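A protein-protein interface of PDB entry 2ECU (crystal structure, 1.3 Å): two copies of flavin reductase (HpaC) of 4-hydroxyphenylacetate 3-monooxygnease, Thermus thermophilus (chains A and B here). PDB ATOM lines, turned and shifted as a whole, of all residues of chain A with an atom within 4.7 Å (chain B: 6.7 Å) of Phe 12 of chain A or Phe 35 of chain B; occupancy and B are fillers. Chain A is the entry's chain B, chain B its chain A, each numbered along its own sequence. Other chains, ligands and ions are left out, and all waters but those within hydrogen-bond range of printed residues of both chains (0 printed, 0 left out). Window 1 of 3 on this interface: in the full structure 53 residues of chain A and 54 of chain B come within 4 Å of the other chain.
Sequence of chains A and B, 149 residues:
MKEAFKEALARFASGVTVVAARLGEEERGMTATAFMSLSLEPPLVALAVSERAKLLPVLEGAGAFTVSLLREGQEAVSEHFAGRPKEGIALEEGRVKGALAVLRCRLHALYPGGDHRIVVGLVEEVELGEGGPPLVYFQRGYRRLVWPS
Among the printed residues, merely in contact across the chains: Ala 8 of chain A with Leu 69 of chain B (3.2 Å), Phe 12 of chain A with Phe 35 of chain B (3.4 Å), Ser 14 of chain A with Ala 13 of chain B (3.4 Å), Ala 13 of chain A with Ser 14 of chain B (3.4 Å), Phe 12 of chain A with Gly 15 of chain B (3.5 Å), Phe 138 of chain A with Pro 134 of chain B (3.5 Å), Leu 9 of chain A with Ser 37 of chain B (3.6 Å), Phe 12 of chain A with Thr 17 of chain B (3.7 Å), Ala 8 of chain A with Leu 103 of chain B (3.7 Å), Met 36 of chain A with Leu 47 of chain B (3.8 Å), Arg 11 of chain A with Leu 69 of chain B (3.9 Å), Met 36 of chain A with Ala 48 of chain B (3.9 Å), Phe 12 of chain A with Thr 33 of chain B (3.9 Å), Phe 12 of chain A with Leu 69 of chain B (3.96 Å) and Met 36 of chain A with Met 36 of chain B (3.99 Å).
The backbone NH of Ala 32 of chain B is in hydrogen-bond range of the backbone carbonyl oxygen of Thr 17 of chain B, at 2.8 Å. The backbone carbonyl oxygen (O) of Ala 34 of chain B is in hydrogen-bond range of the backbone NH (N) of Ala 48 of chain B, 3.1 Å away. The backbone carbonyl oxygen of Met 36 of chain B lies within hydrogen-bond range of the backbone NH of Ala 46 of chain B (2.9 Å). N of Leu 103 of chain B is in hydrogen-bond range of O of Val 67 of chain B, at 2.8 Å. The backbone NH (N) of Leu 100 of chain B is in hydrogen-bond range of the backbone carbonyl oxygen (O) of Leu 69 of chain B (2.8 Å). O of Ser 14 of chain A lies within hydrogen-bond range of N of Tyr 137 of chain A (2.8 Å).
Printed residues of chain B within 4 Å of Ala 13 of chain A: Ser 14 and Gly 15. Val 19 of chain B touches none of the printed residues of chain A. Printed residues of chain A within 4 Å of Ala 34 of chain B: Met 36. Phe 35 of chain B touches just these residues of chain A: Phe 12 and Met 36. Of the printed residues of chain A, Met 36 of chain B touches Met 36 (3.99 Å). Of the printed residues of chain A, Leu 103 of chain B touches Ala 8 (3.7 Å). The nearest residue of chain B that does not touch Phe 12 of chain A is Ser 14 of chain B (4.1 Å). The nearest printed residue of chain B that does not touch Ser 14 of chain A is Phe 12 of chain B (4.1 Å).
The backbone carbonyl oxygen of Ala 13 of chain A sits at hydrogen-bond distance from the backbone NH of Gly 15 of chain B (2.8 Å). N of Phe 35 of chain B is in hydrogen-bond range of SD of Met 36 of chain A (3.7 Å). The backbone carbonyl oxygen of Leu 100 of chain B sits at hydrogen-bond distance from the guanidinium group of Arg 11 of chain A. The side-chain sulfur of Met 36 of chain A sits close to the backbone carbonyl oxygen of Ala 34 of chain B.
Printed residues of chain B that touch a printed residue of chain A: Ala 13, Ser 14, Gly 15, Thr 17, Thr 33, Ala 34, Phe 35, Met 36, Ser 37, Leu 47, Ala 48, Leu 69, Leu 100, Leu 103 and Pro 134. Hydrophobic or aromatic side chains of chain B that line the printed part of chain A: Phe 35, Met 36, Leu 69, Leu 100, Leu 103 and Pro 134. Of the 10 printed residues of chain A, 8 touch a printed residue of chain B. Printed residues of chain A that touch a printed residue of chain B: Ala 8, Leu 9, Arg 11, Phe 12, Ala 13, Ser 14, Met 36 and Phe 138. Hydrophobic or aromatic side chains of chain A that line the printed part of chain B: Ala 8, Leu 9, Phe 12, Met 36 and Phe 138. Along chain A the printed residues that touch a printed residue of chain B span positions 8 to 138. Among the printed residues, 19 pairs touch across the chains. Among the printed residues, no Asp or Glu carboxylate lies within 4 Å of a Lys or Arg side-chain nitrogen of the other chain.
Ala 13 of chain A touches Ser 14 of chain B, and with the chains exchanged Ser 14 of chain A touches Ala 13 of chain B. Met 36 of chain B touches its own counterpart, Met 36 of chain A.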
ATOM      1  N   ALA A   8      27.319   0.341  -0.775  1.00  0.00           N
ATOM      2  CA  ALA A   8      26.274   0.370  -1.791  1.00  0.00           C
ATOM      3  C   ALA A   8      25.696  -1.032  -1.984  1.00  0.00           C
ATOM      4  O   ALA A   8      24.481  -1.204  -2.102  1.00  0.00           O
ATOM      5  CB  ALA A   8      26.836   0.893  -3.105  1.00  0.00           C
ATOM      6  N   LEU A   9      26.567  -2.035  -2.026  1.00  0.00           N
ATOM      7  CA  LEU A   9      26.122  -3.414  -2.198  1.00  0.00           C
ATOM      8  C   LEU A   9      25.329  -3.886  -0.985  1.00  0.00           C
ATOM      9  O   LEU A   9      24.402  -4.686  -1.114  1.00  0.00           O
ATOM     10  CB  LEU A   9      27.318  -4.337  -2.436  1.00  0.00           C
ATOM     11  CG  LEU A   9      28.127  -4.050  -3.702  1.00  0.00           C
ATOM     12  CD1 LEU A   9      29.305  -5.001  -3.786  1.00  0.00           C
ATOM     13  CD2 LEU A   9      27.233  -4.194  -4.914  1.00  0.00           C
ATOM     14  N   ALA A  10      25.695  -3.387   0.191  1.00  0.00           N
ATOM     15  CA  ALA A  10      24.993  -3.741   1.417  1.00  0.00           C
ATOM     16  C   ALA A  10      23.575  -3.181   1.351  1.00  0.00           C
ATOM     17  O   ALA A  10      22.691  -3.615   2.090  1.00  0.00           O
ATOM     18  CB  ALA A  10      25.734  -3.176   2.630  1.00  0.00           C
ATOM     19  N   ARG A  11      23.366  -2.211   0.465  1.00  0.00           N
ATOM     20  CA  ARG A  11      22.055  -1.599   0.308  1.00  0.00           C
ATOM     21  C   ARG A  11      21.186  -2.265  -0.760  1.00  0.00           C
ATOM     22  O   ARG A  11      20.097  -1.783  -1.066  1.00  0.00           O
ATOM     23  CB  ARG A  11      22.198  -0.097   0.041  1.00  0.00           C
ATOM     24  CG  ARG A  11      22.856   0.624   1.211  1.00  0.00           C
ATOM     25  CD  ARG A  11      22.986   2.118   0.987  1.00  0.00           C
ATOM     26  NE  ARG A  11      23.653   2.759   2.120  1.00  0.00           N
ATOM     27  CZ  ARG A  11      23.642   4.069   2.351  1.00  0.00           C
ATOM     28  NH1 ARG A  11      22.997   4.886   1.528  1.00  0.00           N
ATOM     29  NH2 ARG A  11      24.265   4.562   3.414  1.00  0.00           N
ATOM     30  N   PHE A  12      21.674  -3.364  -1.334  1.00  0.00           N
ATOM     31  CA  PHE A  12      20.865  -4.108  -2.291  1.00  0.00           C
ATOM     32  C   PHE A  12      20.384  -5.343  -1.545  1.00  0.00           C
ATOM     33  O   PHE A  12      21.168  -6.244  -1.229  1.00  0.00           O
ATOM     34  CB  PHE A  12      21.643  -4.557  -3.532  1.00  0.00           C
ATOM     35  CG  PHE A  12      20.775  -5.266  -4.542  1.00  0.00           C
ATOM     36  CD1 PHE A  12      19.802  -4.568  -5.252  1.00  0.00           C
ATOM     37  CD2 PHE A  12      20.877  -6.639  -4.727  1.00  0.00           C
ATOM     38  CE1 PHE A  12      18.937  -5.224  -6.132  1.00  0.00           C
ATOM     39  CE2 PHE A  12      20.015  -7.307  -5.604  1.00  0.00           C
ATOM     40  CZ  PHE A  12      19.045  -6.598  -6.305  1.00  0.00           C
ATOM     41  N   ALA A  13      19.093  -5.373  -1.247  1.00  0.00           N
ATOM     42  CA  ALA A  13      18.509  -6.499  -0.536  1.00  0.00           C
ATOM     43  C   ALA A  13      18.380  -7.691  -1.464  1.00  0.00           C
ATOM     44  O   ALA A  13      18.220  -7.541  -2.673  1.00  0.00           O
ATOM     45  CB  ALA A  13      17.139  -6.116   0.004  1.00  0.00           C
ATOM     46  N   SER A  14      18.457  -8.887  -0.902  1.00  0.00           N
ATOM     47  CA  SER A  14      18.303 -10.081  -1.717  1.00  0.00           C
ATOM     48  C   SER A  14      17.953 -11.288  -0.875  1.00  0.00           C
ATOM     49  O   SER A  14      18.092 -11.277   0.350  1.00  0.00           O
ATOM     50  CB  SER A  14      19.589 -10.389  -2.479  1.00  0.00           C
ATOM     51  OG  SER A  14      20.561 -10.941  -1.607  1.00  0.00           O
ATOM     52  N   MET A  36      20.559 -14.409  -9.693  1.00  0.00           N
ATOM     53  CA  MET A  36      19.532 -13.637 -10.372  1.00  0.00           C
ATOM     54  C   MET A  36      18.953 -14.422 -11.531  1.00  0.00           C
ATOM     55  O   MET A  36      19.618 -15.290 -12.094  1.00  0.00           O
ATOM     56  CB  MET A  36      20.098 -12.311 -10.888  1.00  0.00           C
ATOM     57  CG  MET A  36      21.129 -12.436 -11.996  1.00  0.00           C
ATOM     58  SD  MET A  36      21.814 -10.823 -12.394  1.00  0.00           S
ATOM     59  CE  MET A  36      22.840 -11.231 -13.790  1.00  0.00           C
ATOM     60  N   TYR A 137      18.798 -10.832   3.071  1.00  0.00           N
ATOM     61  CA  TYR A 137      20.046 -10.259   3.560  1.00  0.00           C
ATOM     62  C   TYR A 137      20.088  -8.811   3.074  1.00  0.00           C
ATOM     63  O   TYR A 137      19.877  -8.540   1.891  1.00  0.00           O
ATOM     64  CB  TYR A 137      21.267 -11.015   3.032  1.00  0.00           C
ATOM     65  CG  TYR A 137      22.452 -10.871   3.960  1.00  0.00           C
ATOM     66  CD1 TYR A 137      22.458 -11.505   5.204  1.00  0.00           C
ATOM     67  CD2 TYR A 137      23.533 -10.043   3.640  1.00  0.00           C
ATOM     68  CE1 TYR A 137      23.498 -11.317   6.108  1.00  0.00           C
ATOM     69  CE2 TYR A 137      24.585  -9.851   4.542  1.00  0.00           C
ATOM     70  CZ  TYR A 137      24.555 -10.489   5.772  1.00  0.00           C
ATOM     71  OH  TYR A 137      25.573 -10.289   6.682  1.00  0.00           O
ATOM     72  N   PHE A 138      20.363  -7.887   3.988  1.00  0.00           N
ATOM     73  CA  PHE A 138      20.402  -6.466   3.667  1.00  0.00           C
ATOM     74  C   PHE A 138      21.109  -5.757   4.811  1.00  0.00           C
ATOM     75  O   PHE A 138      20.878  -6.068   5.977  1.00  0.00           O
ATOM     76  CB  PHE A 138      18.966  -5.940   3.512  1.00  0.00           C
ATOM     77  CG  PHE A 138      18.861  -4.440   3.357  1.00  0.00           C
ATOM     78  CD1 PHE A 138      19.157  -3.816   2.147  1.00  0.00           C
ATOM     79  CD2 PHE A 138      18.443  -3.653   4.426  1.00  0.00           C
ATOM     80  CE1 PHE A 138      19.032  -2.431   2.003  1.00  0.00           C
ATOM     81  CE2 PHE A 138      18.315  -2.270   4.295  1.00  0.00           C
ATOM     82  CZ  PHE A 138      18.610  -1.658   3.081  1.00  0.00           C
ATOM     83  N   PHE B  12      12.418 -15.553  -5.085  1.00  0.00           N
ATOM     84  CA  PHE B  12      13.720 -14.984  -4.760  1.00  0.00           C
ATOM     85  C   PHE B  12      13.486 -13.489  -4.579  1.00  0.00           C
ATOM     86  O   PHE B  12      13.203 -12.766  -5.538  1.00  0.00           O
ATOM     87  CB  PHE B  12      14.763 -15.188  -5.862  1.00  0.00           C
ATOM     88  CG  PHE B  12      16.133 -14.692  -5.470  1.00  0.00           C
ATOM     89  CD1 PHE B  12      16.871 -15.357  -4.495  1.00  0.00           C
ATOM     90  CD2 PHE B  12      16.660 -13.524  -6.019  1.00  0.00           C
ATOM     91  CE1 PHE B  12      18.106 -14.873  -4.066  1.00  0.00           C
ATOM     92  CE2 PHE B  12      17.899 -13.031  -5.596  1.00  0.00           C
ATOM     93  CZ  PHE B  12      18.619 -13.705  -4.620  1.00  0.00           C
ATOM     94  N   ALA B  13      13.584 -13.033  -3.338  1.00  0.00           N
ATOM     95  CA  ALA B  13      13.382 -11.629  -3.032  1.00  0.00           C
ATOM     96  C   ALA B  13      14.582 -10.831  -3.507  1.00  0.00           C
ATOM     97  O   ALA B  13      15.702 -11.330  -3.537  1.00  0.00           O
ATOM     98  CB  ALA B  13      13.209 -11.449  -1.536  1.00  0.00           C
ATOM     99  N   SER B  14      14.347  -9.585  -3.889  1.00  0.00           N
ATOM    100  CA  SER B  14      15.454  -8.747  -4.317  1.00  0.00           C
ATOM    101  C   SER B  14      15.095  -7.285  -4.251  1.00  0.00           C
ATOM    102  O   SER B  14      13.921  -6.917  -4.200  1.00  0.00           O
ATOM    103  CB  SER B  14      15.860  -9.067  -5.752  1.00  0.00           C
ATOM    104  OG  SER B  14      14.920  -8.521  -6.657  1.00  0.00           O
ATOM    105  N   GLY B  15      16.126  -6.455  -4.226  1.00  0.00           N
ATOM    106  CA  GLY B  15      15.900  -5.031  -4.249  1.00  0.00           C
ATOM    107  C   GLY B  15      15.502  -4.722  -5.683  1.00  0.00           C
ATOM    108  O   GLY B  15      15.454  -5.621  -6.527  1.00  0.00           O
ATOM    109  N   VAL B  16      15.213  -3.458  -5.958  1.00  0.00           N
ATOM    110  CA  VAL B  16      14.816  -3.035  -7.291  1.00  0.00           C
ATOM    111  C   VAL B  16      15.749  -1.917  -7.718  1.00  0.00           C
ATOM    112  O   VAL B  16      16.005  -0.988  -6.951  1.00  0.00           O
ATOM    113  CB  VAL B  16      13.357  -2.525  -7.301  1.00  0.00           C
ATOM    114  CG1 VAL B  16      12.935  -2.165  -8.722  1.00  0.00           C
ATOM    115  CG2 VAL B  16      12.432  -3.591  -6.720  1.00  0.00           C
ATOM    116  N   THR B  17      16.271  -2.023  -8.935  1.00  0.00           N
ATOM    117  CA  THR B  17      17.186  -1.015  -9.449  1.00  0.00           C
ATOM    118  C   THR B  17      16.656  -0.405 -10.730  1.00  0.00           C
ATOM    119  O   THR B  17      15.702  -0.905 -11.336  1.00  0.00           O
ATOM    120  CB  THR B  17      18.576  -1.613  -9.807  1.00  0.00           C
ATOM    121  OG1 THR B  17      18.509  -2.242 -11.097  1.00  0.00           O
ATOM    122  CG2 THR B  17      19.008  -2.647  -8.775  1.00  0.00           C
ATOM    123  N   VAL B  19      18.483   0.858 -14.195  1.00  0.00           N
ATOM    124  CA  VAL B  19      19.729   0.898 -14.950  1.00  0.00           C
ATOM    125  C   VAL B  19      19.538   1.949 -16.030  1.00  0.00           C
ATOM    126  O   VAL B  19      18.535   1.932 -16.743  1.00  0.00           O
ATOM    127  CB  VAL B  19      20.022  -0.455 -15.621  1.00  0.00           C
ATOM    128  CG1 VAL B  19      21.402  -0.435 -16.263  1.00  0.00           C
ATOM    129  CG2 VAL B  19      19.914  -1.573 -14.602  1.00  0.00           C
ATOM    130  N   ALA B  32      15.173  -2.953 -13.189  1.00  0.00           N
ATOM    131  CA  ALA B  32      15.702  -4.307 -13.181  1.00  0.00           C
ATOM    132  C   ALA B  32      15.897  -4.855 -11.777  1.00  0.00           C
ATOM    133  O   ALA B  32      16.412  -4.168 -10.893  1.00  0.00           O
ATOM    134  CB  ALA B  32      17.032  -4.357 -13.930  1.00  0.00           C
ATOM    135  N   THR B  33      15.469  -6.096 -11.578  1.00  0.00           N
ATOM    136  CA  THR B  33      15.665  -6.774 -10.305  1.00  0.00           C
ATOM    137  C   THR B  33      16.847  -7.723 -10.496  1.00  0.00           C
ATOM    138  O   THR B  33      17.455  -8.177  -9.528  1.00  0.00           O
ATOM    139  CB  THR B  33      14.430  -7.590  -9.885  1.00  0.00           C
ATOM    140  OG1 THR B  33      13.914  -8.293 -11.018  1.00  0.00           O
ATOM    141  CG2 THR B  33      13.360  -6.679  -9.309  1.00  0.00           C
ATOM    142  N   ALA B  34      17.173  -8.006 -11.757  1.00  0.00           N
ATOM    143  CA  ALA B  34      18.285  -8.890 -12.095  1.00  0.00           C
ATOM    144  C   ALA B  34      19.604  -8.123 -12.001  1.00  0.00           C
ATOM    145  O   ALA B  34      20.173  -7.691 -13.009  1.00  0.00           O
ATOM    146  CB  ALA B  34      18.097  -9.456 -13.500  1.00  0.00           C
ATOM    147  N   PHE B  35      20.074  -7.956 -10.769  1.00  0.00           N
ATOM    148  CA  PHE B  35      21.310  -7.251 -10.466  1.00  0.00           C
ATOM    149  C   PHE B  35      22.010  -8.011  -9.354  1.00  0.00           C
ATOM    150  O   PHE B  35      21.354  -8.539  -8.455  1.00  0.00           O
ATOM    151  CB  PHE B  35      20.995  -5.832  -9.977  1.00  0.00           C
ATOM    152  CG  PHE B  35      22.148  -5.159  -9.283  1.00  0.00           C
ATOM    153  CD1 PHE B  35      23.113  -4.471 -10.010  1.00  0.00           C
ATOM    154  CD2 PHE B  35      22.288  -5.239  -7.899  1.00  0.00           C
ATOM    155  CE1 PHE B  35      24.199  -3.875  -9.370  1.00  0.00           C
ATOM    156  CE2 PHE B  35      23.372  -4.647  -7.250  1.00  0.00           C
ATOM    157  CZ  PHE B  35      24.328  -3.964  -7.988  1.00  0.00           C
ATOM    158  N   MET B  36      23.336  -8.073  -9.404  1.00  0.00           N
ATOM    159  CA  MET B  36      24.074  -8.743  -8.343  1.00  0.00           C
ATOM    160  C   MET B  36      25.519  -8.277  -8.302  1.00  0.00           C
ATOM    161  O   MET B  36      26.077  -7.857  -9.324  1.00  0.00           O
ATOM    162  CB  MET B  36      24.037 -10.265  -8.521  1.00  0.00           C
ATOM    163  CG  MET B  36      24.785 -10.789  -9.734  1.00  0.00           C
ATOM    164  SD  MET B  36      24.595 -12.572  -9.902  1.00  0.00           S
ATOM    165  CE  MET B  36      25.661 -12.898 -11.287  1.00  0.00           C
ATOM    166  N   SER B  37      26.115  -8.307  -7.115  1.00  0.00           N
ATOM    167  CA  SER B  37      27.512  -7.934  -6.997  1.00  0.00           C
ATOM    168  C   SER B  37      28.264  -9.072  -7.680  1.00  0.00           C
ATOM    169  O   SER B  37      27.788 -10.213  -7.715  1.00  0.00           O
ATOM    170  CB  SER B  37      27.926  -7.817  -5.530  1.00  0.00           C
ATOM    171  OG  SER B  37      27.729  -9.033  -4.843  1.00  0.00           O
ATOM    172  N   VAL B  45      29.922  -5.476 -11.044  1.00  0.00           N
ATOM    173  CA  VAL B  45      28.541  -5.852 -10.783  1.00  0.00           C
ATOM    174  C   VAL B  45      28.016  -6.432 -12.092  1.00  0.00           C
ATOM    175  O   VAL B  45      28.557  -6.149 -13.169  1.00  0.00           O
ATOM    176  CB  VAL B  45      27.651  -4.655 -10.357  1.00  0.00           C
ATOM    177  CG1 VAL B  45      28.135  -4.096  -9.037  1.00  0.00           C
ATOM    178  CG2 VAL B  45      27.651  -3.584 -11.428  1.00  0.00           C
ATOM    179  N   ALA B  46      26.989  -7.270 -12.001  1.00  0.00           N
ATOM    180  CA  ALA B  46      26.404  -7.883 -13.189  1.00  0.00           C
ATOM    181  C   ALA B  46      24.899  -7.670 -13.213  1.00  0.00           C
ATOM    182  O   ALA B  46      24.248  -7.616 -12.166  1.00  0.00           O
ATOM    183  CB  ALA B  46      26.710  -9.371 -13.217  1.00  0.00           C
ATOM    184  N   LEU B  47      24.352  -7.546 -14.415  1.00  0.00           N
ATOM    185  CA  LEU B  47      22.923  -7.350 -14.577  1.00  0.00           C
ATOM    186  C   LEU B  47      22.441  -8.085 -15.810  1.00  0.00           C
ATOM    187  O   LEU B  47      23.226  -8.401 -16.703  1.00  0.00           O
ATOM    188  CB  LEU B  47      22.591  -5.866 -14.730  1.00  0.00           C
ATOM    189  CG  LEU B  47      23.037  -4.918 -13.619  1.00  0.00           C
ATOM    190  CD1 LEU B  47      24.505  -4.559 -13.797  1.00  0.00           C
ATOM    191  CD2 LEU B  47      22.190  -3.665 -13.666  1.00  0.00           C
ATOM    192  N   ALA B  48      21.144  -8.369 -15.846  1.00  0.00           N
ATOM    193  CA  ALA B  48      20.542  -9.032 -16.991  1.00  0.00           C
ATOM    194  C   ALA B  48      19.669  -7.999 -17.680  1.00  0.00           C
ATOM    195  O   ALA B  48      18.754  -7.447 -17.074  1.00  0.00           O
ATOM    196  CB  ALA B  48      19.703 -10.218 -16.541  1.00  0.00           C
ATOM    197  N   VAL B  67      23.530   2.485 -12.095  1.00  0.00           N
ATOM    198  CA  VAL B  67      22.593   1.581 -11.448  1.00  0.00           C
ATOM    199  C   VAL B  67      22.155   2.264 -10.162  1.00  0.00           C
ATOM    200  O   VAL B  67      22.986   2.563  -9.311  1.00  0.00           O
ATOM    201  CB  VAL B  67      23.241   0.218 -11.097  1.00  0.00           C
ATOM    202  CG1 VAL B  67      22.206  -0.698 -10.436  1.00  0.00           C
ATOM    203  CG2 VAL B  67      23.805  -0.429 -12.349  1.00  0.00           C
ATOM    204  N   LEU B  69      19.800   2.063  -6.762  1.00  0.00           N
ATOM    205  CA  LEU B  69      19.109   1.132  -5.870  1.00  0.00           C
ATOM    206  C   LEU B  69      17.957   1.881  -5.215  1.00  0.00           C
ATOM    207  O   LEU B  69      18.172   2.810  -4.434  1.00  0.00           O
ATOM    208  CB  LEU B  69      20.075   0.616  -4.800  1.00  0.00           C
ATOM    209  CG  LEU B  69      21.393   0.027  -5.318  1.00  0.00           C
ATOM    210  CD1 LEU B  69      22.158  -0.597  -4.165  1.00  0.00           C
ATOM    211  CD2 LEU B  69      21.120  -1.010  -6.395  1.00  0.00           C
ATOM    212  N   LEU B 100      18.881   4.818  -2.630  1.00  0.00           N
ATOM    213  CA  LEU B 100      19.727   4.369  -1.530  1.00  0.00           C
ATOM    214  C   LEU B 100      21.193   4.470  -1.931  1.00  0.00           C
ATOM    215  O   LEU B 100      22.061   4.756  -1.104  1.00  0.00           O
ATOM    216  CB  LEU B 100      19.407   2.922  -1.162  1.00  0.00           C
ATOM    217  CG  LEU B 100      18.369   2.744  -0.055  1.00  0.00           C
ATOM    218  CD1 LEU B 100      17.866   1.313  -0.074  1.00  0.00           C
ATOM    219  CD2 LEU B 100      18.979   3.093   1.297  1.00  0.00           C
ATOM    220  N   LEU B 103      25.572   3.458  -8.527  1.00  0.00           N
ATOM    221  CA  LEU B 103      26.853   2.949  -8.990  1.00  0.00           C
ATOM    222  C   LEU B 103      27.029   3.447 -10.415  1.00  0.00           C
ATOM    223  O   LEU B 103      26.182   3.184 -11.268  1.00  0.00           O
ATOM    224  CB  LEU B 103      26.864   1.422  -9.005  1.00  0.00           C
ATOM    225  CG  LEU B 103      26.690   0.696  -7.674  1.00  0.00           C
ATOM    226  CD1 LEU B 103      26.758  -0.807  -7.915  1.00  0.00           C
ATOM    227  CD2 LEU B 103      27.772   1.121  -6.701  1.00  0.00           C
ATOM    228  N   PRO B 134      14.786  -0.514   1.993  1.00  0.00           N
ATOM    229  CA  PRO B 134      14.753  -0.614   0.531  1.00  0.00           C
ATOM    230  C   PRO B 134      13.415  -0.961  -0.102  1.00  0.00           C
ATOM    231  O   PRO B 134      12.463  -1.332   0.580  1.00  0.00           O
ATOM    232  CB  PRO B 134      15.758  -1.718   0.273  1.00  0.00           C
ATOM    233  CG  PRO B 134      15.382  -2.702   1.368  1.00  0.00           C
ATOM    234  CD  PRO B 134      15.133  -1.819   2.593  1.00  0.00           C
ATOM    235  N   LEU B 135      13.356  -0.823  -1.424  1.00  0.00           N
ATOM    236  CA  LEU B 135      12.176  -1.222  -2.174  1.00  0.00           C
ATOM    237  C   LEU B 135      12.498  -2.686  -2.481  1.00  0.00           C
ATOM    238  O   LEU B 135      13.592  -2.999  -2.970  1.00  0.00           O
ATOM    239  CB  LEU B 135      12.047  -0.433  -3.481  1.00  0.00           C
ATOM    240  CG  LEU B 135      10.809  -0.785  -4.312  1.00  0.00           C
ATOM    241  CD1 LEU B 135       9.543  -0.481  -3.513  1.00  0.00           C
ATOM    242  CD2 LEU B 135      10.825   0.002  -5.615  1.00  0.00           C
